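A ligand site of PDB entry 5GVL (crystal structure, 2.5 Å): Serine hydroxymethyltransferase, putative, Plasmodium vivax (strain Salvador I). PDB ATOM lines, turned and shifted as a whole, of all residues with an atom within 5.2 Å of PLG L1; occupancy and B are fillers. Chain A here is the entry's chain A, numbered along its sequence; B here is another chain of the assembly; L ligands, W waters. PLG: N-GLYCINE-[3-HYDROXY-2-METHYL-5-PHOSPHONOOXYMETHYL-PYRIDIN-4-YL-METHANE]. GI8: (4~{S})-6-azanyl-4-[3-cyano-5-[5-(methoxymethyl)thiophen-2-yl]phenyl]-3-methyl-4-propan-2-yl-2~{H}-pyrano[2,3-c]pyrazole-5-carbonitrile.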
ATOM      1  N   ILE A  32     -36.105  19.758  25.027  1.00  0.00           N
ATOM      2  CA  ILE A  32     -35.039  20.703  25.428  1.00  0.00           C
ATOM      3  C   ILE A  32     -34.006  20.855  24.303  1.00  0.00           C
ATOM      4  O   ILE A  32     -33.277  19.913  23.955  1.00  0.00           O
ATOM      5  CB  ILE A  32     -34.361  20.327  26.757  1.00  0.00           C
ATOM      6  CG1 ILE A  32     -35.379  20.383  27.913  1.00  0.00           C
ATOM      7  CG2 ILE A  32     -33.196  21.258  27.051  1.00  0.00           C
ATOM      8  CD1 ILE A  32     -35.027  19.494  29.071  1.00  0.00           C
ATOM      9  N   SER A  34     -31.224  22.241  23.912  1.00  0.00           N
ATOM     10  CA  SER A  34     -29.817  22.005  24.229  1.00  0.00           C
ATOM     11  C   SER A  34     -29.479  20.575  24.661  1.00  0.00           C
ATOM     12  O   SER A  34     -28.337  20.293  25.054  1.00  0.00           O
ATOM     13  CB  SER A  34     -29.391  22.960  25.333  1.00  0.00           C
ATOM     14  OG  SER A  34     -30.273  22.836  26.423  1.00  0.00           O
ATOM     15  N   SER A 100     -16.472  22.981  29.648  1.00  0.00           N
ATOM     16  CA  SER A 100     -17.856  23.238  29.304  1.00  0.00           C
ATOM     17  C   SER A 100     -17.942  24.565  28.557  1.00  0.00           C
ATOM     18  O   SER A 100     -16.977  25.338  28.538  1.00  0.00           O
ATOM     19  CB  SER A 100     -18.721  23.275  30.574  1.00  0.00           C
ATOM     20  OG  SER A 100     -19.889  22.460  30.453  1.00  0.00           O
ATOM     21  N   GLY A 101     -19.091  24.844  27.961  1.00  0.00           N
ATOM     22  CA  GLY A 101     -19.288  26.039  27.158  1.00  0.00           C
ATOM     23  C   GLY A 101     -19.063  27.373  27.839  1.00  0.00           C
ATOM     24  O   GLY A 101     -18.580  28.330  27.199  1.00  0.00           O
ATOM     25  N   SER A 102     -19.404  27.452  29.124  1.00  0.00           N
ATOM     26  CA  SER A 102     -19.296  28.691  29.892  1.00  0.00           C
ATOM     27  C   SER A 102     -17.824  28.990  30.151  1.00  0.00           C
ATOM     28  O   SER A 102     -17.387  30.131  29.997  1.00  0.00           O
ATOM     29  CB  SER A 102     -20.101  28.630  31.198  1.00  0.00           C
ATOM     30  OG  SER A 102     -21.482  28.389  30.997  1.00  0.00           O
ATOM     31  N   ALA A 103     -17.062  27.958  30.526  1.00  0.00           N
ATOM     32  CA  ALA A 103     -15.607  28.084  30.733  1.00  0.00           C
ATOM     33  C   ALA A 103     -14.860  28.507  29.468  1.00  0.00           C
ATOM     34  O   ALA A 103     -14.145  29.491  29.518  1.00  0.00           O
ATOM     35  CB  ALA A 103     -15.012  26.808  31.327  1.00  0.00           C
ATOM     36  N   ASN A 105     -15.972  30.006  26.713  1.00  0.00           N
ATOM     37  CA  ASN A 105     -16.324  31.402  26.424  1.00  0.00           C
ATOM     38  C   ASN A 105     -15.566  32.416  27.293  1.00  0.00           C
ATOM     39  O   ASN A 105     -15.056  33.405  26.759  1.00  0.00           O
ATOM     40  CB  ASN A 105     -17.837  31.632  26.507  1.00  0.00           C
ATOM     41  CG  ASN A 105     -18.577  31.117  25.289  1.00  0.00           C
ATOM     42  OD1 ASN A 105     -17.991  30.558  24.389  1.00  0.00           O
ATOM     43  ND2 ASN A 105     -19.887  31.291  25.275  1.00  0.00           N
ATOM     44  N   HIS A 129     -26.567  34.217  25.377  1.00  0.00           N
ATOM     45  CA  HIS A 129     -26.118  33.459  26.533  1.00  0.00           C
ATOM     46  C   HIS A 129     -25.718  34.334  27.721  1.00  0.00           C
ATOM     47  O   HIS A 129     -25.458  35.528  27.564  1.00  0.00           O
ATOM     48  CB  HIS A 129     -25.011  32.450  26.210  1.00  0.00           C
ATOM     49  CG  HIS A 129     -24.910  31.355  27.231  1.00  0.00           C
ATOM     50  ND1 HIS A 129     -23.892  31.311  28.161  1.00  0.00           N
ATOM     51  CD2 HIS A 129     -25.730  30.328  27.526  1.00  0.00           C
ATOM     52  CE1 HIS A 129     -24.067  30.272  28.951  1.00  0.00           C
ATOM     53  NE2 HIS A 129     -25.177  29.661  28.596  1.00  0.00           N
ATOM     54  N   THR A 131     -22.906  33.952  29.274  1.00  0.00           N
ATOM     55  CA  THR A 131     -21.488  34.234  29.027  1.00  0.00           C
ATOM     56  C   THR A 131     -21.221  35.239  27.899  1.00  0.00           C
ATOM     57  O   THR A 131     -20.076  35.417  27.500  1.00  0.00           O
ATOM     58  CB  THR A 131     -20.698  32.948  28.759  1.00  0.00           C
ATOM     59  OG1 THR A 131     -21.265  32.264  27.634  1.00  0.00           O
ATOM     60  CG2 THR A 131     -20.698  32.043  29.987  1.00  0.00           C
ATOM     61  N   HIS A 132     -22.279  35.894  27.404  1.00  0.00           N
ATOM     62  CA  HIS A 132     -22.166  36.932  26.382  1.00  0.00           C
ATOM     63  C   HIS A 132     -22.253  38.333  26.974  1.00  0.00           C
ATOM     64  O   HIS A 132     -22.631  39.302  26.302  1.00  0.00           O
ATOM     65  CB  HIS A 132     -23.210  36.733  25.267  1.00  0.00           C
ATOM     66  CG  HIS A 132     -23.090  35.428  24.550  1.00  0.00           C
ATOM     67  ND1 HIS A 132     -23.958  35.060  23.544  1.00  0.00           N
ATOM     68  CD2 HIS A 132     -22.224  34.389  24.677  1.00  0.00           C
ATOM     69  CE1 HIS A 132     -23.648  33.860  23.092  1.00  0.00           C
ATOM     70  NE2 HIS A 132     -22.585  33.438  23.763  1.00  0.00           N
ATOM     71  N   GLY A 181     -24.115  34.264  17.565  1.00  0.00           N
ATOM     72  CA  GLY A 181     -24.330  32.816  17.809  1.00  0.00           C
ATOM     73  C   GLY A 181     -24.922  32.676  19.203  1.00  0.00           C
ATOM     74  O   GLY A 181     -24.389  33.250  20.159  1.00  0.00           O
ATOM     75  N   TYR A 182     -26.045  31.960  19.327  1.00  0.00           N
ATOM     76  CA  TYR A 182     -26.901  32.194  20.496  1.00  0.00           C
ATOM     77  C   TYR A 182     -27.496  30.970  21.159  1.00  0.00           C
ATOM     78  O   TYR A 182     -27.368  29.855  20.650  1.00  0.00           O
ATOM     79  CB  TYR A 182     -28.011  33.204  20.145  1.00  0.00           C
ATOM     80  CG  TYR A 182     -27.540  34.398  19.357  1.00  0.00           C
ATOM     81  CD1 TYR A 182     -26.911  35.484  19.979  1.00  0.00           C
ATOM     82  CD2 TYR A 182     -27.729  34.451  17.954  1.00  0.00           C
ATOM     83  CE1 TYR A 182     -26.479  36.577  19.248  1.00  0.00           C
ATOM     84  CE2 TYR A 182     -27.309  35.562  17.211  1.00  0.00           C
ATOM     85  CZ  TYR A 182     -26.685  36.615  17.865  1.00  0.00           C
ATOM     86  OH  TYR A 182     -26.266  37.715  17.158  1.00  0.00           O
ATOM     87  N   THR A 183     -28.119  31.192  22.317  1.00  0.00           N
ATOM     88  CA  THR A 183     -28.728  30.112  23.106  1.00  0.00           C
ATOM     89  C   THR A 183     -30.164  29.801  22.688  1.00  0.00           C
ATOM     90  O   THR A 183     -30.540  28.623  22.611  1.00  0.00           O
ATOM     91  CB  THR A 183     -28.577  30.295  24.637  1.00  0.00           C
ATOM     92  OG1 THR A 183     -29.838  30.123  25.303  1.00  0.00           O
ATOM     93  CG2 THR A 183     -28.111  31.602  24.958  1.00  0.00           C
ATOM     94  N   ASP A 208     -20.311  31.924  18.653  1.00  0.00           N
ATOM     95  CA  ASP A 208     -20.561  30.826  19.575  1.00  0.00           C
ATOM     96  C   ASP A 208     -21.664  30.032  18.912  1.00  0.00           C
ATOM     97  O   ASP A 208     -22.807  30.493  18.815  1.00  0.00           O
ATOM     98  CB  ASP A 208     -20.992  31.378  20.943  1.00  0.00           C
ATOM     99  CG  ASP A 208     -21.375  30.303  21.953  1.00  0.00           C
ATOM    100  OD1 ASP A 208     -21.529  29.108  21.628  1.00  0.00           O
ATOM    101  OD2 ASP A 208     -21.532  30.685  23.135  1.00  0.00           O
ATOM    102  N   SER A 210     -22.658  26.764  19.690  1.00  0.00           N
ATOM    103  CA  SER A 210     -23.021  25.588  20.507  1.00  0.00           C
ATOM    104  C   SER A 210     -24.357  24.998  20.115  1.00  0.00           C
ATOM    105  O   SER A 210     -24.486  23.783  19.975  1.00  0.00           O
ATOM    106  CB  SER A 210     -23.037  25.936  21.992  1.00  0.00           C
ATOM    107  OG  SER A 210     -21.888  26.672  22.382  1.00  0.00           O
ATOM    108  N   HIS A 211     -25.350  25.872  19.925  1.00  0.00           N
ATOM    109  CA  HIS A 211     -26.672  25.425  19.516  1.00  0.00           C
ATOM    110  C   HIS A 211     -26.827  24.909  18.094  1.00  0.00           C
ATOM    111  O   HIS A 211     -27.680  24.061  17.822  1.00  0.00           O
ATOM    112  CB  HIS A 211     -27.725  26.490  19.836  1.00  0.00           C
ATOM    113  CG  HIS A 211     -28.373  26.265  21.165  1.00  0.00           C
ATOM    114  ND1 HIS A 211     -29.406  25.373  21.339  1.00  0.00           N
ATOM    115  CD2 HIS A 211     -28.063  26.732  22.395  1.00  0.00           C
ATOM    116  CE1 HIS A 211     -29.740  25.337  22.619  1.00  0.00           C
ATOM    117  NE2 HIS A 211     -28.941  26.158  23.276  1.00  0.00           N
ATOM    118  N   THR A 234     -20.010  24.189  22.532  1.00  0.00           N
ATOM    119  CA  THR A 234     -20.080  23.014  23.383  1.00  0.00           C
ATOM    120  C   THR A 234     -20.159  21.774  22.490  1.00  0.00           C
ATOM    121  O   THR A 234     -20.417  21.894  21.304  1.00  0.00           O
ATOM    122  CB  THR A 234     -21.324  23.076  24.282  1.00  0.00           C
ATOM    123  OG1 THR A 234     -22.497  23.245  23.481  1.00  0.00           O
ATOM    124  CG2 THR A 234     -21.219  24.196  25.257  1.00  0.00           C
ATOM    125  N   HIS A 236     -22.041  18.795  23.658  1.00  0.00           N
ATOM    126  CA  HIS A 236     -23.122  17.956  24.204  1.00  0.00           C
ATOM    127  C   HIS A 236     -24.499  18.216  23.615  1.00  0.00           C
ATOM    128  O   HIS A 236     -25.430  17.430  23.847  1.00  0.00           O
ATOM    129  CB  HIS A 236     -23.192  18.088  25.738  1.00  0.00           C
ATOM    130  CG  HIS A 236     -22.936  19.470  26.255  1.00  0.00           C
ATOM    131  ND1 HIS A 236     -21.671  19.996  26.362  1.00  0.00           N
ATOM    132  CD2 HIS A 236     -23.781  20.432  26.701  1.00  0.00           C
ATOM    133  CE1 HIS A 236     -21.741  21.217  26.865  1.00  0.00           C
ATOM    134  NE2 HIS A 236     -23.013  21.513  27.077  1.00  0.00           N
ATOM    135  N   LYS A 237     -24.639  19.299  22.866  1.00  0.00           N
ATOM    136  CA  LYS A 237     -25.935  19.675  22.296  1.00  0.00           C
ATOM    137  C   LYS A 237     -26.188  18.940  20.974  1.00  0.00           C
ATOM    138  O   LYS A 237     -26.087  17.690  20.895  1.00  0.00           O
ATOM    139  CB  LYS A 237     -26.033  21.185  22.137  1.00  0.00           C
ATOM    140  CG  LYS A 237     -25.949  21.962  23.439  1.00  0.00           C
ATOM    141  CD  LYS A 237     -26.104  23.444  23.182  1.00  0.00           C
ATOM    142  CE  LYS A 237     -25.999  24.248  24.462  1.00  0.00           C
ATOM    143  NZ  LYS A 237     -24.638  24.265  25.064  1.00  0.00           N
ATOM    144  N   ARG A 243     -20.227  16.280  27.497  1.00  0.00           N
ATOM    145  CA  ARG A 243     -20.269  17.647  27.981  1.00  0.00           C
ATOM    146  C   ARG A 243     -18.849  18.216  27.994  1.00  0.00           C
ATOM    147  O   ARG A 243     -18.059  17.909  28.883  1.00  0.00           O
ATOM    148  CB  ARG A 243     -20.883  17.740  29.379  1.00  0.00           C
ATOM    149  CG  ARG A 243     -22.248  17.106  29.499  1.00  0.00           C
ATOM    150  CD  ARG A 243     -22.908  17.506  30.818  1.00  0.00           C
ATOM    151  NE  ARG A 243     -23.513  18.828  30.727  1.00  0.00           N
ATOM    152  CZ  ARG A 243     -24.718  19.075  30.227  1.00  0.00           C
ATOM    153  NH1 ARG A 243     -25.489  18.078  29.776  1.00  0.00           N
ATOM    154  NH2 ARG A 243     -25.161  20.331  30.177  1.00  0.00           N
ATOM    155  N   ARG A 371     -39.161  27.320  25.150  1.00  0.00           N
ATOM    156  CA  ARG A 371     -38.325  26.955  24.032  1.00  0.00           C
ATOM    157  C   ARG A 371     -38.343  25.435  23.848  1.00  0.00           C
ATOM    158  O   ARG A 371     -38.286  24.687  24.822  1.00  0.00           O
ATOM    159  CB  ARG A 371     -36.907  27.490  24.227  1.00  0.00           C
ATOM    160  CG  ARG A 371     -35.976  27.302  23.036  1.00  0.00           C
ATOM    161  CD  ARG A 371     -34.522  27.404  23.449  1.00  0.00           C
ATOM    162  NE  ARG A 371     -34.121  26.401  24.457  1.00  0.00           N
ATOM    163  CZ  ARG A 371     -32.923  26.343  25.033  1.00  0.00           C
ATOM    164  NH1 ARG A 371     -31.966  27.209  24.718  1.00  0.00           N
ATOM    165  NH2 ARG A 371     -32.672  25.409  25.924  1.00  0.00           N
ATOM    166  N   TYR B  54     -29.558  18.589  31.195  1.00  0.00           N
ATOM    167  CA  TYR B  54     -29.288  19.997  31.489  1.00  0.00           C
ATOM    168  C   TYR B  54     -30.077  20.344  32.736  1.00  0.00           C
ATOM    169  O   TYR B  54     -31.286  20.136  32.778  1.00  0.00           O
ATOM    170  CB  TYR B  54     -29.727  20.923  30.332  1.00  0.00           C
ATOM    171  CG  TYR B  54     -28.581  21.724  29.781  1.00  0.00           C
ATOM    172  CD1 TYR B  54     -27.963  22.751  30.530  1.00  0.00           C
ATOM    173  CD2 TYR B  54     -28.052  21.414  28.540  1.00  0.00           C
ATOM    174  CE1 TYR B  54     -26.880  23.450  30.016  1.00  0.00           C
ATOM    175  CE2 TYR B  54     -26.973  22.090  28.021  1.00  0.00           C
ATOM    176  CZ  TYR B  54     -26.389  23.098  28.757  1.00  0.00           C
ATOM    177  OH  TYR B  54     -25.314  23.734  28.190  1.00  0.00           O
ATOM    178  N   GLU B  56     -29.362  23.411  34.941  1.00  0.00           N
ATOM    179  CA  GLU B  56     -28.907  24.714  35.415  1.00  0.00           C
ATOM    180  C   GLU B  56     -29.701  25.216  36.624  1.00  0.00           C
ATOM    181  O   GLU B  56     -30.930  25.141  36.641  1.00  0.00           O
ATOM    182  CB  GLU B  56     -28.953  25.727  34.289  1.00  0.00           C
ATOM    183  CG  GLU B  56     -27.588  26.017  33.721  1.00  0.00           C
ATOM    184  CD  GLU B  56     -27.606  26.787  32.422  1.00  0.00           C
ATOM    185  OE1 GLU B  56     -27.825  26.150  31.381  1.00  0.00           O
ATOM    186  OE2 GLU B  56     -27.355  28.007  32.428  1.00  0.00           O
ATOM    187  N   TYR B  64     -35.067  23.965  33.916  1.00  0.00           N
ATOM    188  CA  TYR B  64     -35.571  22.957  32.991  1.00  0.00           C
ATOM    189  C   TYR B  64     -36.500  21.995  33.722  1.00  0.00           C
ATOM    190  O   TYR B  64     -36.356  21.775  34.949  1.00  0.00           O
ATOM    191  CB  TYR B  64     -34.434  22.170  32.290  1.00  0.00           C
ATOM    192  CG  TYR B  64     -33.343  23.047  31.705  1.00  0.00           C
ATOM    193  CD1 TYR B  64     -33.498  23.650  30.454  1.00  0.00           C
ATOM    194  CD2 TYR B  64     -32.158  23.293  32.419  1.00  0.00           C
ATOM    195  CE1 TYR B  64     -32.515  24.486  29.929  1.00  0.00           C
ATOM    196  CE2 TYR B  64     -31.158  24.116  31.899  1.00  0.00           C
ATOM    197  CZ  TYR B  64     -31.331  24.703  30.651  1.00  0.00           C
ATOM    198  OH  TYR B  64     -30.350  25.519  30.139  1.00  0.00           O
ATOM    199  N   GLN B 270     -20.209  29.094  35.801  1.00  0.00           N
ATOM    200  CA  GLN B 270     -20.614  27.886  35.095  1.00  0.00           C
ATOM    201  C   GLN B 270     -22.045  27.957  34.529  1.00  0.00           C
ATOM    202  O   GLN B 270     -22.798  28.880  34.829  1.00  0.00           O
ATOM    203  CB  GLN B 270     -20.425  26.618  35.956  1.00  0.00           C
ATOM    204  CG  GLN B 270     -18.994  26.316  36.379  1.00  0.00           C
ATOM    205  CD  GLN B 270     -18.808  24.982  37.099  1.00  0.00           C
ATOM    206  OE1 GLN B 270     -17.684  24.548  37.335  1.00  0.00           O
ATOM    207  NE2 GLN B 270     -19.911  24.317  37.427  1.00  0.00           N
ATOM    208  N   GLY B 271     -22.371  26.999  33.671  1.00  0.00           N
ATOM    209  CA  GLY B 271     -23.707  26.795  33.161  1.00  0.00           C
ATOM    210  C   GLY B 271     -24.227  25.471  33.677  1.00  0.00           C
ATOM    211  O   GLY B 271     -24.304  25.257  34.891  1.00  0.00           O
ATOM    212  N   GLY B 272     -24.579  24.576  32.754  1.00  0.00           N
ATOM    213  CA  GLY B 272     -25.121  23.264  33.097  1.00  0.00           C
ATOM    214  C   GLY B 272     -24.134  22.464  33.935  1.00  0.00           C
ATOM    215  O   GLY B 272     -22.955  22.390  33.601  1.00  0.00           O
ATOM    216  N   HIS B 274     -22.332  19.061  35.449  1.00  0.00           N
ATOM    217  CA  HIS B 274     -21.989  17.769  34.866  1.00  0.00           C
ATOM    218  C   HIS B 274     -22.415  16.668  35.836  1.00  0.00           C
ATOM    219  O   HIS B 274     -21.696  16.307  36.776  1.00  0.00           O
ATOM    220  CB  HIS B 274     -20.506  17.679  34.503  1.00  0.00           C
ATOM    221  CG  HIS B 274     -20.099  18.553  33.364  1.00  0.00           C
ATOM    222  ND1 HIS B 274     -18.919  18.375  32.671  1.00  0.00           N
ATOM    223  CD2 HIS B 274     -20.706  19.631  32.779  1.00  0.00           C
ATOM    224  CE1 HIS B 274     -18.817  19.289  31.729  1.00  0.00           C
ATOM    225  NE2 HIS B 274     -19.888  20.063  31.773  1.00  0.00           N
HETATM  226  N1  PLG L   1     -23.093  28.977  24.764  1.00  0.00           N
HETATM  227  C2  PLG L   1     -24.371  28.868  24.358  1.00  0.00           C
HETATM  228  C2A PLG L   1     -24.797  29.537  23.065  1.00  0.00           C
HETATM  229  C3  PLG L   1     -25.324  28.060  25.197  1.00  0.00           C
HETATM  230  O3  PLG L   1     -26.613  27.913  24.813  1.00  0.00           O
HETATM  231  C4  PLG L   1     -24.819  27.413  26.451  1.00  0.00           C
HETATM  232  C4A PLG L   1     -25.719  26.612  27.384  1.00  0.00           C
HETATM  233  C5  PLG L   1     -23.374  27.651  26.763  1.00  0.00           C
HETATM  234  C6  PLG L   1     -22.614  28.423  25.886  1.00  0.00           C
HETATM  235  C5A PLG L   1     -22.697  27.116  28.003  1.00  0.00           C
HETATM  236  OP4 PLG L   1     -22.638  25.696  28.032  1.00  0.00           O
HETATM  237  P   PLG L   1     -22.347  24.955  29.413  1.00  0.00           P
HETATM  238  OP1 PLG L   1     -21.359  25.750  30.221  1.00  0.00           O
HETATM  239  OP2 PLG L   1     -23.730  24.939  30.034  1.00  0.00           O
HETATM  240  OP3 PLG L   1     -21.797  23.634  28.950  1.00  0.00           O
HETATM  241  C   PLG L   1     -29.368  25.991  26.923  1.00  0.00           C
HETATM  242  O   PLG L   1     -30.108  25.131  27.437  1.00  0.00           O
HETATM  243  OXT PLG L   1     -29.509  26.371  25.743  1.00  0.00           O
HETATM  244  CA  PLG L   1     -28.239  26.580  27.725  1.00  0.00           C
HETATM  245  N   PLG L   1     -27.073  26.505  26.887  1.00  0.00           N
HETATM  246  N9  GI8 L   2     -34.387  32.612  27.699  1.00  0.00           N
HETATM  247  C8  GI8 L   2     -33.337  32.225  27.997  1.00  0.00           C
HETATM  248  C3  GI8 L   2     -32.185  31.785  28.341  1.00  0.00           C
HETATM  249  C2  GI8 L   2     -31.084  32.268  27.682  1.00  0.00           C
HETATM  250  N7  GI8 L   2     -31.184  33.157  26.704  1.00  0.00           N
HETATM  251  O1  GI8 L   2     -29.734  31.842  28.006  1.00  0.00           O
HETATM  252  C6  GI8 L   2     -29.517  31.043  29.089  1.00  0.00           C
HETATM  253  N12 GI8 L   2     -28.316  30.690  29.568  1.00  0.00           N
HETATM  254  N11 GI8 L   2     -28.603  29.846  30.664  1.00  0.00           N
HETATM  255  C10 GI8 L   2     -29.925  29.686  30.870  1.00  0.00           C
HETATM  256  C13 GI8 L   2     -30.524  28.861  31.990  1.00  0.00           C
HETATM  257  C5  GI8 L   2     -30.637  30.476  29.820  1.00  0.00           C
HETATM  258  C4  GI8 L   2     -32.096  30.751  29.488  1.00  0.00           C
HETATM  259  C14 GI8 L   2     -32.815  29.444  29.046  1.00  0.00           C
HETATM  260  C16 GI8 L   2     -33.187  28.451  30.154  1.00  0.00           C
HETATM  261  C15 GI8 L   2     -32.099  28.684  27.926  1.00  0.00           C
HETATM  262  C17 GI8 L   2     -32.760  31.433  30.684  1.00  0.00           C
HETATM  263  C18 GI8 L   2     -34.147  31.538  30.763  1.00  0.00           C
HETATM  264  C19 GI8 L   2     -34.787  32.168  31.820  1.00  0.00           C
HETATM  265  C23 GI8 L   2     -36.064  32.221  31.834  1.00  0.00           C
HETATM  266  N24 GI8 L   2     -37.215  32.269  31.858  1.00  0.00           N
HETATM  267  C22 GI8 L   2     -32.026  32.021  31.712  1.00  0.00           C
HETATM  268  C21 GI8 L   2     -32.656  32.650  32.791  1.00  0.00           C
HETATM  269  C20 GI8 L   2     -34.044  32.745  32.848  1.00  0.00           C
HETATM  270  C25 GI8 L   2     -31.769  33.211  33.835  1.00  0.00           C
HETATM  271  S29 GI8 L   2     -32.153  34.756  34.481  1.00  0.00           S
HETATM  272  C28 GI8 L   2     -30.803  34.792  35.536  1.00  0.00           C
HETATM  273  C27 GI8 L   2     -30.068  33.626  35.371  1.00  0.00           C
HETATM  274  C26 GI8 L   2     -30.613  32.742  34.431  1.00  0.00           C
HETATM  275  C30 GI8 L   2     -30.649  36.032  36.387  1.00  0.00           C
HETATM  276  O31 GI8 L   2     -30.853  35.797  37.778  1.00  0.00           O
HETATM  277  C32 GI8 L   2     -29.806  35.081  38.459  1.00  0.00           C
HETATM  278  O   HOH W   1     -20.585  24.811  32.857  1.00  0.00           O
HETATM  279  O   HOH W   2     -23.011  21.707  30.837  1.00  0.00           O
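ND2 of Asn 105 touches N1 of PLG L1 (3.99 Å). His 129 touches PLG L1. O of Tyr 182 touches C2A of PLG L1, at 3.5 Å. Thr 183 touches PLG L1 (CB to O3, 3.1 Å). Ser 210 touches PLG L1 (OG to N1, 3.5 Å). CG2 of Thr 234 touches OP4 of PLG L1, 3.5 Å away. Lys 237 touches PLG L1 (NZ to C4, 3.4 Å). Glu 56 of chain B touches PLG L1. Gly 271 of chain B touches PLG L1. Hydrophobic or aromatic side chains within 4 Å of PLG L1: His 129, His 211, His 236, Tyr 54 of chain B and Tyr 64 of chain B. 20 residues have an atom within 4 Å of PLG L1: Ser 34, Ser 100, Gly 101, Ser 102, Asn 105, His 129, Tyr 182, Thr 183, Asp 208, Ser 210, His 211, Thr 234, His 236, Lys 237, Arg 371, Tyr 54 of chain B, Glu 56 of chain B, Tyr 64 of chain B, Gly 271 of chain B and Gly 272 of chain B.
Water W1 lies within hydrogen-bond range of OP1 of PLG L1, N of Gly 271 of chain B, OG of Ser 100 and O of Gly 272 of chain B. Water W2 lies within hydrogen-bond range of NH2 of Arg 243, O of Gly 272 of chain B, OP3 of PLG L1 and OG of Ser 100.
OG of Ser 34 sits at hydrogen-bond distance from O of PLG L1, at 2.5 Å. OXT of PLG L1 lies within hydrogen-bond range of NE2 of His 211 (2.5 Å). The side-chain hydroxyl of Ser 100 sits at hydrogen-bond distance from an oxygen (OP3) of PLG L1 (2.7 Å). An oxygen (OP2) of PLG L1 lies within hydrogen-bond range of the side-chain hydroxyl (OH) of Tyr 54 of chain B. The side-chain hydroxyl (OH) of Tyr 64 of chain B sits at hydrogen-bond distance from an oxygen (O) of PLG L1 (2.7 Å). N of Ser 102 is in hydrogen-bond range of OP1 of PLG L1. The side-chain hydroxyl (OG) of Ser 102 is in hydrogen-bond range of an oxygen (OP1) of PLG L1 (2.8 Å). OXT of PLG L1 is in salt-bridge range of NH1 of Arg 371 (2.8 Å). A nitrogen (N1) of PLG L1 lies within hydrogen-bond range of the side-chain carboxylate of Asp 208 (2.8 Å). N of Gly 272 of chain B lies within hydrogen-bond range of OP2 of PLG L1. NE2 of His 236 sits at hydrogen-bond distance from OP3 of PLG L1. An oxygen (OP3) of PLG L1 is in hydrogen-bond range of the backbone NH (N) of Gly 101, at 3.1 Å. An oxygen (O1) of GI8 L2 sits at hydrogen-bond distance from the side-chain hydroxyl (OG1) of Thr 183 (3.2 Å). A nitrogen (N12) of GI8 L2 sits close to a ring nitrogen (NE2) of His 129 (3.4 Å). The side-chain carboxylate (OE2) of Glu 56 of chain B sits at hydrogen-bond distance from a nitrogen (N11) of GI8 L2 (2.8 Å).
A ring nitrogen (NE2) of His 211 is in hydrogen-bond range of the backbone carbonyl oxygen (O) of Thr 183, 3.0 Å away. NE2 of His 274 of chain B sits at hydrogen-bond distance from OG of Ser 100. A ring nitrogen (NE2) of His 236 sits at hydrogen-bond distance from the side-chain hydroxyl (OH) of Tyr 54 of chain B (3.4 Å). OH of Tyr 64 of chain B lies within hydrogen-bond range of OE1 of Glu 56 of chain B (2.9 Å). NH1 of Arg 371 sits at hydrogen-bond distance from O of Thr 183, at 2.9 Å. The side-chain hydroxyl (OG) of Ser 210 sits at hydrogen-bond distance from the side-chain carboxylate (OD1) of Asp 208 (2.6 Å). The side-chain amide nitrogen of Asn 105 lies within hydrogen-bond range of the side-chain carboxylate of Asp 208 (2.8 Å). The side-chain hydroxyl (OG1) of Thr 131 lies within hydrogen-bond range of a ring nitrogen (ND1) of His 129 (2.8 Å).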
